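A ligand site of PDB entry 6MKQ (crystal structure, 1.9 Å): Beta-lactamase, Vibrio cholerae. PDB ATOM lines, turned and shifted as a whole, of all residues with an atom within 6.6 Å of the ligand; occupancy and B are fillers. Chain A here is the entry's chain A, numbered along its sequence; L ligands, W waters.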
ATOM      1  N   LEU A  41       3.379 -22.129   8.029  1.00  0.00           N
ATOM      2  CA  LEU A  41       4.409 -21.422   7.272  1.00  0.00           C
ATOM      3  C   LEU A  41       5.408 -20.722   8.201  1.00  0.00           C
ATOM      4  O   LEU A  41       6.608 -20.667   7.891  1.00  0.00           O
ATOM      5  CB  LEU A  41       3.766 -20.402   6.340  1.00  0.00           C
ATOM      6  CG  LEU A  41       3.183 -20.914   5.031  1.00  0.00           C
ATOM      7  CD1 LEU A  41       2.168 -19.933   4.478  1.00  0.00           C
ATOM      8  CD2 LEU A  41       4.298 -21.157   4.030  1.00  0.00           C
ATOM      9  N   CYS A  42       4.926 -20.176   9.325  1.00  0.00           N
ATOM     10  CA  CYS A  42       5.760 -19.343  10.179  1.00  0.00           C
ATOM     11  C   CYS A  42       6.372 -18.243   9.317  1.00  0.00           C
ATOM     12  O   CYS A  42       5.703 -17.732   8.421  1.00  0.00           O
ATOM     13  CB  CYS A  42       6.836 -20.171  10.882  1.00  0.00           C
ATOM     14  SG  CYS A  42       6.206 -21.702  11.675  1.00  0.00           S
ATOM     15  N   SER A  43       7.635 -17.881   9.564  1.00  0.00           N
ATOM     16  CA  SER A  43       8.281 -16.799   8.823  1.00  0.00           C
ATOM     17  C   SER A  43       8.543 -17.127   7.343  1.00  0.00           C
ATOM     18  O   SER A  43       8.915 -16.218   6.590  1.00  0.00           O
ATOM     19  CB  SER A  43       9.628 -16.462   9.477  1.00  0.00           C
ATOM     20  OG  SER A  43       9.516 -15.631  10.617  1.00  0.00           O
ATOM     21  N   SER A  44       8.363 -18.373   6.923  1.00  0.00           N
ATOM     22  CA  SER A  44       8.859 -18.795   5.618  1.00  0.00           C
ATOM     23  C   SER A  44       8.127 -18.110   4.463  1.00  0.00           C
ATOM     24  O   SER A  44       8.685 -18.056   3.367  1.00  0.00           O
ATOM     25  CB  SER A  44       8.800 -20.322   5.498  1.00  0.00           C
ATOM     26  OG  SER A  44       7.486 -20.807   5.273  1.00  0.00           O
ATOM     27  N   LYS A  46       7.918 -15.079   4.098  1.00  0.00           N
ATOM     28  CA  LYS A  46       8.532 -13.769   3.881  1.00  0.00           C
ATOM     29  C   LYS A  46       9.441 -13.751   2.651  1.00  0.00           C
ATOM     30  O   LYS A  46       9.648 -12.682   2.075  1.00  0.00           O
ATOM     31  CB  LYS A  46       9.319 -13.355   5.130  1.00  0.00           C
ATOM     32  CG  LYS A  46       8.430 -12.980   6.330  1.00  0.00           C
ATOM     33  CD  LYS A  46       9.252 -12.875   7.612  1.00  0.00           C
ATOM     34  CE  LYS A  46       8.404 -12.526   8.827  1.00  0.00           C
ATOM     35  NZ  LYS A  46       9.075 -12.944  10.086  1.00  0.00           N
ATOM     36  N   PRO A  77       7.764  -7.560  17.778  1.00  0.00           N
ATOM     37  CA  PRO A  77       8.956  -8.329  18.172  1.00  0.00           C
ATOM     38  C   PRO A  77       9.637  -8.927  16.951  1.00  0.00           C
ATOM     39  O   PRO A  77       8.999  -9.215  15.936  1.00  0.00           O
ATOM     40  CB  PRO A  77       8.387  -9.425  19.090  1.00  0.00           C
ATOM     41  CG  PRO A  77       7.169  -8.781  19.703  1.00  0.00           C
ATOM     42  CD  PRO A  77       6.589  -7.904  18.596  1.00  0.00           C
ATOM     43  N   HIS A  78      10.972  -9.061  17.040  1.00  0.00           N
ATOM     44  CA  HIS A  78      11.797  -9.662  15.986  1.00  0.00           C
ATOM     45  C   HIS A  78      11.782  -8.800  14.715  1.00  0.00           C
ATOM     46  O   HIS A  78      11.477  -9.254  13.610  1.00  0.00           O
ATOM     47  CB  HIS A  78      11.340 -11.088  15.711  1.00  0.00           C
ATOM     48  CG  HIS A  78      11.436 -11.975  16.916  1.00  0.00           C
ATOM     49  ND1 HIS A  78      12.640 -12.353  17.468  1.00  0.00           N
ATOM     50  CD2 HIS A  78      10.470 -12.539  17.680  1.00  0.00           C
ATOM     51  CE1 HIS A  78      12.409 -13.119  18.533  1.00  0.00           C
ATOM     52  NE2 HIS A  78      11.109 -13.244  18.674  1.00  0.00           N
ATOM     53  N   TYR A 102      16.561 -11.158   7.166  1.00  0.00           N
ATOM     54  CA  TYR A 102      16.586 -11.065   8.615  1.00  0.00           C
ATOM     55  C   TYR A 102      15.274 -11.495   9.243  1.00  0.00           C
ATOM     56  O   TYR A 102      15.101 -11.376  10.467  1.00  0.00           O
ATOM     57  CB  TYR A 102      16.915  -9.639   9.057  1.00  0.00           C
ATOM     58  CG  TYR A 102      18.215  -9.113   8.511  1.00  0.00           C
ATOM     59  CD1 TYR A 102      18.297  -8.589   7.227  1.00  0.00           C
ATOM     60  CD2 TYR A 102      19.363  -9.136   9.276  1.00  0.00           C
ATOM     61  CE1 TYR A 102      19.476  -8.112   6.730  1.00  0.00           C
ATOM     62  CE2 TYR A 102      20.558  -8.656   8.776  1.00  0.00           C
ATOM     63  CZ  TYR A 102      20.610  -8.145   7.508  1.00  0.00           C
ATOM     64  OH  TYR A 102      21.804  -7.652   7.010  1.00  0.00           O
ATOM     65  N   SER A 103      14.319 -11.982   8.441  1.00  0.00           N
ATOM     66  CA  SER A 103      13.033 -12.457   8.931  1.00  0.00           C
ATOM     67  C   SER A 103      12.280 -11.375   9.693  1.00  0.00           C
ATOM     68  O   SER A 103      11.528 -11.669  10.627  1.00  0.00           O
ATOM     69  CB  SER A 103      13.209 -13.711   9.802  1.00  0.00           C
ATOM     70  OG  SER A 103      11.997 -14.419   9.923  1.00  0.00           O
ATOM     71  N   ASP A 104      12.452 -10.122   9.278  1.00  0.00           N
ATOM     72  CA  ASP A 104      11.972  -8.972  10.038  1.00  0.00           C
ATOM     73  C   ASP A 104      10.447  -8.911  10.024  1.00  0.00           C
ATOM     74  O   ASP A 104       9.834  -8.832   8.958  1.00  0.00           O
ATOM     75  CB  ASP A 104      12.572  -7.702   9.428  1.00  0.00           C
ATOM     76  CG  ASP A 104      12.402  -6.480  10.305  1.00  0.00           C
ATOM     77  OD1 ASP A 104      11.249  -6.045  10.515  1.00  0.00           O
ATOM     78  OD2 ASP A 104      13.437  -5.935  10.763  1.00  0.00           O
ATOM     79  N   ASN A 105       9.851  -8.919  11.227  1.00  0.00           N
ATOM     80  CA  ASN A 105       8.397  -8.950  11.325  1.00  0.00           C
ATOM     81  C   ASN A 105       7.767  -7.605  10.986  1.00  0.00           C
ATOM     82  O   ASN A 105       6.738  -7.542  10.301  1.00  0.00           O
ATOM     83  CB  ASN A 105       7.978  -9.376  12.730  1.00  0.00           C
ATOM     84  CG  ASN A 105       7.887 -10.875  12.881  1.00  0.00           C
ATOM     85  OD1 ASN A 105       7.664 -11.579  11.903  1.00  0.00           O
ATOM     86  ND2 ASN A 105       8.059 -11.354  14.098  1.00  0.00           N
ATOM     87  N   GLU A 140       1.523 -10.846  11.188  1.00  0.00           N
ATOM     88  CA  GLU A 140       2.453 -11.044  12.292  1.00  0.00           C
ATOM     89  C   GLU A 140       1.888 -10.357  13.539  1.00  0.00           C
ATOM     90  O   GLU A 140       1.404  -9.228  13.461  1.00  0.00           O
ATOM     91  CB  GLU A 140       3.831 -10.469  11.950  1.00  0.00           C
ATOM     92  CG  GLU A 140       4.590 -11.218  10.876  1.00  0.00           C
ATOM     93  CD  GLU A 140       5.063 -12.592  11.314  1.00  0.00           C
ATOM     94  OE1 GLU A 140       4.859 -12.946  12.494  1.00  0.00           O
ATOM     95  OE2 GLU A 140       5.626 -13.321  10.474  1.00  0.00           O
ATOM     96  N   LEU A 141       1.923 -11.030  14.693  1.00  0.00           N
ATOM     97  CA  LEU A 141       2.548 -12.336  14.883  1.00  0.00           C
ATOM     98  C   LEU A 141       1.532 -13.458  15.063  1.00  0.00           C
ATOM     99  O   LEU A 141       1.900 -14.609  15.325  1.00  0.00           O
ATOM    100  CB  LEU A 141       3.482 -12.289  16.111  1.00  0.00           C
ATOM    101  CG  LEU A 141       4.926 -11.839  15.858  1.00  0.00           C
ATOM    102  CD1 LEU A 141       4.980 -10.356  15.562  1.00  0.00           C
ATOM    103  CD2 LEU A 141       5.872 -12.177  17.015  1.00  0.00           C
ATOM    104  N   LEU A 143      -0.104 -15.100  13.014  1.00  0.00           N
ATOM    105  CA  LEU A 143      -0.029 -16.194  12.050  1.00  0.00           C
ATOM    106  C   LEU A 143       0.825 -17.352  12.549  1.00  0.00           C
ATOM    107  O   LEU A 143       0.858 -18.395  11.893  1.00  0.00           O
ATOM    108  CB  LEU A 143       0.500 -15.683  10.705  1.00  0.00           C
ATOM    109  CG  LEU A 143       1.904 -15.067  10.646  1.00  0.00           C
ATOM    110  CD1 LEU A 143       2.958 -16.140  10.458  1.00  0.00           C
ATOM    111  CD2 LEU A 143       1.997 -14.038   9.523  1.00  0.00           C
ATOM    112  N   ASN A 144       1.512 -17.202  13.684  1.00  0.00           N
ATOM    113  CA  ASN A 144       2.469 -18.188  14.167  1.00  0.00           C
ATOM    114  C   ASN A 144       1.876 -19.201  15.151  1.00  0.00           C
ATOM    115  O   ASN A 144       2.643 -19.964  15.738  1.00  0.00           O
ATOM    116  CB  ASN A 144       3.654 -17.481  14.857  1.00  0.00           C
ATOM    117  CG  ASN A 144       4.489 -16.651  13.900  1.00  0.00           C
ATOM    118  OD1 ASN A 144       5.169 -17.184  13.032  1.00  0.00           O
ATOM    119  ND2 ASN A 144       4.451 -15.343  14.073  1.00  0.00           N
ATOM    120  N   ASN A 188      20.842 -14.766   3.015  1.00  0.00           N
ATOM    121  CA  ASN A 188      20.016 -14.957   4.206  1.00  0.00           C
ATOM    122  C   ASN A 188      20.903 -15.187   5.422  1.00  0.00           C
ATOM    123  O   ASN A 188      21.912 -15.885   5.351  1.00  0.00           O
ATOM    124  CB  ASN A 188      19.083 -16.155   4.022  1.00  0.00           C
ATOM    125  CG  ASN A 188      18.160 -16.334   5.209  1.00  0.00           C
ATOM    126  OD1 ASN A 188      17.487 -15.396   5.639  1.00  0.00           O
ATOM    127  ND2 ASN A 188      18.140 -17.544   5.768  1.00  0.00           N
ATOM    128  N   THR A 190      19.856 -16.375   8.604  1.00  0.00           N
ATOM    129  CA  THR A 190      19.276 -17.148   9.690  1.00  0.00           C
ATOM    130  C   THR A 190      19.296 -18.656   9.492  1.00  0.00           C
ATOM    131  O   THR A 190      18.667 -19.364  10.289  1.00  0.00           O
ATOM    132  CB  THR A 190      17.815 -16.746   9.937  1.00  0.00           C
ATOM    133  OG1 THR A 190      17.045 -17.103   8.770  1.00  0.00           O
ATOM    134  CG2 THR A 190      17.667 -15.261  10.204  1.00  0.00           C
ATOM    135  N   GLY A 191      19.952 -19.158   8.464  1.00  0.00           N
ATOM    136  CA  GLY A 191      19.777 -20.574   8.151  1.00  0.00           C
ATOM    137  C   GLY A 191      20.978 -21.475   8.339  1.00  0.00           C
ATOM    138  O   GLY A 191      20.994 -22.603   7.839  1.00  0.00           O
ATOM    139  N   ARG A 194      20.305 -25.162   9.594  1.00  0.00           N
ATOM    140  CA  ARG A 194      19.300 -26.011   8.950  1.00  0.00           C
ATOM    141  C   ARG A 194      19.875 -26.569   7.652  1.00  0.00           C
ATOM    142  O   ARG A 194      20.865 -27.298   7.698  1.00  0.00           O
ATOM    143  CB  ARG A 194      18.020 -25.214   8.770  1.00  0.00           C
ATOM    144  CG  ARG A 194      17.442 -24.918  10.155  1.00  0.00           C
ATOM    145  CD  ARG A 194      16.111 -24.207  10.219  1.00  0.00           C
ATOM    146  NE  ARG A 194      15.817 -23.901  11.619  1.00  0.00           N
ATOM    147  CZ  ARG A 194      14.751 -23.209  12.041  1.00  0.00           C
ATOM    148  NH1 ARG A 194      13.867 -22.734  11.174  1.00  0.00           N
ATOM    149  NH2 ARG A 194      14.591 -22.976  13.336  1.00  0.00           N
ATOM    150  N   LYS A 208      15.315 -19.626   3.120  1.00  0.00           N
ATOM    151  CA  LYS A 208      14.494 -18.858   4.044  1.00  0.00           C
ATOM    152  C   LYS A 208      13.934 -19.792   5.122  1.00  0.00           C
ATOM    153  O   LYS A 208      13.278 -20.781   4.780  1.00  0.00           O
ATOM    154  CB  LYS A 208      13.329 -18.156   3.343  1.00  0.00           C
ATOM    155  CG  LYS A 208      12.454 -17.348   4.293  1.00  0.00           C
ATOM    156  CD  LYS A 208      13.162 -16.081   4.755  1.00  0.00           C
ATOM    157  CE  LYS A 208      12.435 -15.405   5.937  1.00  0.00           C
ATOM    158  NZ  LYS A 208      12.717 -16.088   7.227  1.00  0.00           N
ATOM    159  N   THR A 209      14.158 -19.431   6.378  1.00  0.00           N
ATOM    160  CA  THR A 209      13.749 -20.220   7.532  1.00  0.00           C
ATOM    161  C   THR A 209      12.397 -19.769   8.065  1.00  0.00           C
ATOM    162  O   THR A 209      11.887 -18.691   7.733  1.00  0.00           O
ATOM    163  CB  THR A 209      14.779 -20.093   8.652  1.00  0.00           C
ATOM    164  OG1 THR A 209      15.003 -18.700   8.918  1.00  0.00           O
ATOM    165  CG2 THR A 209      16.101 -20.740   8.288  1.00  0.00           C
ATOM    166  N   GLY A 210      11.819 -20.607   8.923  1.00  0.00           N
ATOM    167  CA  GLY A 210      10.639 -20.235   9.694  1.00  0.00           C
ATOM    168  C   GLY A 210      10.610 -20.954  11.037  1.00  0.00           C
ATOM    169  O   GLY A 210      10.981 -22.124  11.113  1.00  0.00           O
ATOM    170  N   THR A 211      10.179 -20.257  12.096  1.00  0.00           N
ATOM    171  CA  THR A 211      10.200 -20.793  13.461  1.00  0.00           C
ATOM    172  C   THR A 211       9.041 -20.153  14.226  1.00  0.00           C
ATOM    173  O   THR A 211       9.188 -19.064  14.790  1.00  0.00           O
ATOM    174  CB  THR A 211      11.532 -20.514  14.158  1.00  0.00           C
ATOM    175  OG1 THR A 211      12.629 -20.956  13.357  1.00  0.00           O
ATOM    176  CG2 THR A 211      11.571 -21.197  15.518  1.00  0.00           C
ATOM    177  N   CYS A 212       7.908 -20.859  14.284  1.00  0.00           N
ATOM    178  CA  CYS A 212       6.690 -20.239  14.799  1.00  0.00           C
ATOM    179  C   CYS A 212       6.812 -19.873  16.280  1.00  0.00           C
ATOM    180  O   CYS A 212       6.184 -18.903  16.722  1.00  0.00           O
ATOM    181  CB  CYS A 212       5.487 -21.158  14.602  1.00  0.00           C
ATOM    182  SG  CYS A 212       4.719 -21.128  12.959  1.00  0.00           S
ATOM    183  N   GLY A 213       7.589 -20.622  17.055  1.00  0.00           N
ATOM    184  CA  GLY A 213       7.584 -20.459  18.491  1.00  0.00           C
ATOM    185  C   GLY A 213       6.496 -21.238  19.192  1.00  0.00           C
ATOM    186  O   GLY A 213       6.330 -21.089  20.409  1.00  0.00           O
ATOM    187  N   ASN A 219      11.007 -24.687  10.034  1.00  0.00           N
ATOM    188  CA  ASN A 219      11.137 -25.076   8.640  1.00  0.00           C
ATOM    189  C   ASN A 219      12.266 -24.304   7.970  1.00  0.00           C
ATOM    190  O   ASN A 219      12.835 -23.367   8.538  1.00  0.00           O
ATOM    191  CB  ASN A 219       9.798 -24.884   7.897  1.00  0.00           C
ATOM    192  CG  ASN A 219       9.261 -23.464   8.028  1.00  0.00           C
ATOM    193  OD1 ASN A 219       9.836 -22.517   7.510  1.00  0.00           O
ATOM    194  ND2 ASN A 219       8.142 -23.315   8.736  1.00  0.00           N
HETATM  195  O1  LIG L   1       8.979 -17.430  11.807  1.00  0.00           O
HETATM  196  C1  LIG L   1       9.474 -16.326  11.819  1.00  0.00           C
HETATM  197  N1  LIG L   1       9.898 -15.689  12.823  1.00  0.00           N
HETATM  198  C2  LIG L   1      10.592 -14.398  12.723  1.00  0.00           C
HETATM  199  C3  LIG L   1       9.619 -16.204  14.145  1.00  0.00           C
HETATM  200  C4  LIG L   1       8.550 -15.280  14.782  1.00  0.00           C
HETATM  201  O2  LIG L   1       7.985 -14.445  14.151  1.00  0.00           O
HETATM  202  N2  LIG L   1       8.255 -15.435  16.194  1.00  0.00           N
HETATM  203  C5  LIG L   1      10.875 -16.251  14.972  1.00  0.00           C
HETATM  204  C6  LIG L   1      11.717 -14.958  14.881  1.00  0.00           C
HETATM  205  C7  LIG L   1      11.916 -14.398  13.468  1.00  0.00           C
HETATM  206  N3  LIG L   1      12.871 -15.187  12.665  1.00  0.00           N
HETATM  207  O3  LIG L   1      13.087 -16.510  13.089  1.00  0.00           O
HETATM  208  S1  LIG L   1      13.240 -17.404  11.670  1.00  0.00           S
HETATM  209  O4  LIG L   1      14.439 -17.104  10.885  1.00  0.00           O
HETATM  210  O5  LIG L   1      13.334 -18.848  11.849  1.00  0.00           O
HETATM  211  O6  LIG L   1      12.135 -17.221  10.752  1.00  0.00           O
HETATM  212  O   HOH W   1      15.764 -14.706  13.791  1.00  0.00           O
HETATM  213  O   HOH W   2      10.024 -18.320  17.620  1.00  0.00           O
HETATM  214  O   HOH W   3       7.393 -14.121  18.845  1.00  0.00           O
HETATM  215  O   HOH W   4       6.698 -15.448  11.721  1.00  0.00           O
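The side-chain hydroxyl of Ser 43 is covalently linked to a carbon (C1) of the ligand.
O4 of the ligand is in hydrogen-bond range of OG1 of Thr 209 (2.6 Å).
OG1 of Thr 190 is in hydrogen-bond range of O4 of the ligand, at 3.4 Å.
The backbone NH of Thr 211 sits at hydrogen-bond distance from an oxygen (O1) of the ligand, 3.1 Å away.
The side-chain hydroxyl of Thr 211 sits at hydrogen-bond distance from an oxygen (O5) of the ligand, at 2.7 Å.
An oxygen (O2) of the ligand lies within hydrogen-bond range of the side-chain amide nitrogen of Asn 105 (3.1 Å).
O1 of the ligand sits close to N of Ser 43 (2.7 Å).
OG of Ser 103 is in hydrogen-bond range of O6 of the ligand (2.9 Å).
The side-chain amino group (NZ) of Lys 208 lies within salt-bridge range of an oxygen (O6) of the ligand.
The guanidinium group of Arg 194 lies within salt-bridge range of an oxygen (O5) of the ligand, at 3.98 Å.
OG of Ser 43 is in hydrogen-bond range of NZ of Lys 46, at 2.8 Å.
The guanidinium group (NH1) of Arg 194 sits at hydrogen-bond distance from the backbone carbonyl oxygen (O) of Asn 219 (2.9 Å).
The backbone NH (N) of Asn 105 sits at hydrogen-bond distance from the backbone carbonyl oxygen (O) of His 78 (2.9 Å).
The side-chain hydroxyl (OG) of Ser 103 lies within hydrogen-bond range of the side-chain amino group (NZ) of Lys 208, at 3.3 Å.
ND2 of Asn 144 lies within hydrogen-bond range of O of Leu 141, at 2.9 Å.
ND2 of Asn 105 lies within hydrogen-bond range of O of Pro 77 (3.0 Å).
NH2 of Arg 194 sits at hydrogen-bond distance from OG1 of Thr 211 (2.8 Å).
The side-chain sulfur (SG) of Cys 42 forms a disulfide with the side-chain sulfur (SG) of Cys 212.
Cys 42 touches the ligand.
Lys 46 touches the ligand (NZ to C2, 3.4 Å).
His 78 touches the ligand.
Glu 140 touches the ligand (OE1 to O2, 3.8 Å).
Asn 144 touches the ligand (ND2 to O2, 3.6 Å).
Gly 210 touches the ligand (CA to O6, 3.5 Å).
Of the 26 residues printed, 14 come within 4 Å of the ligand.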
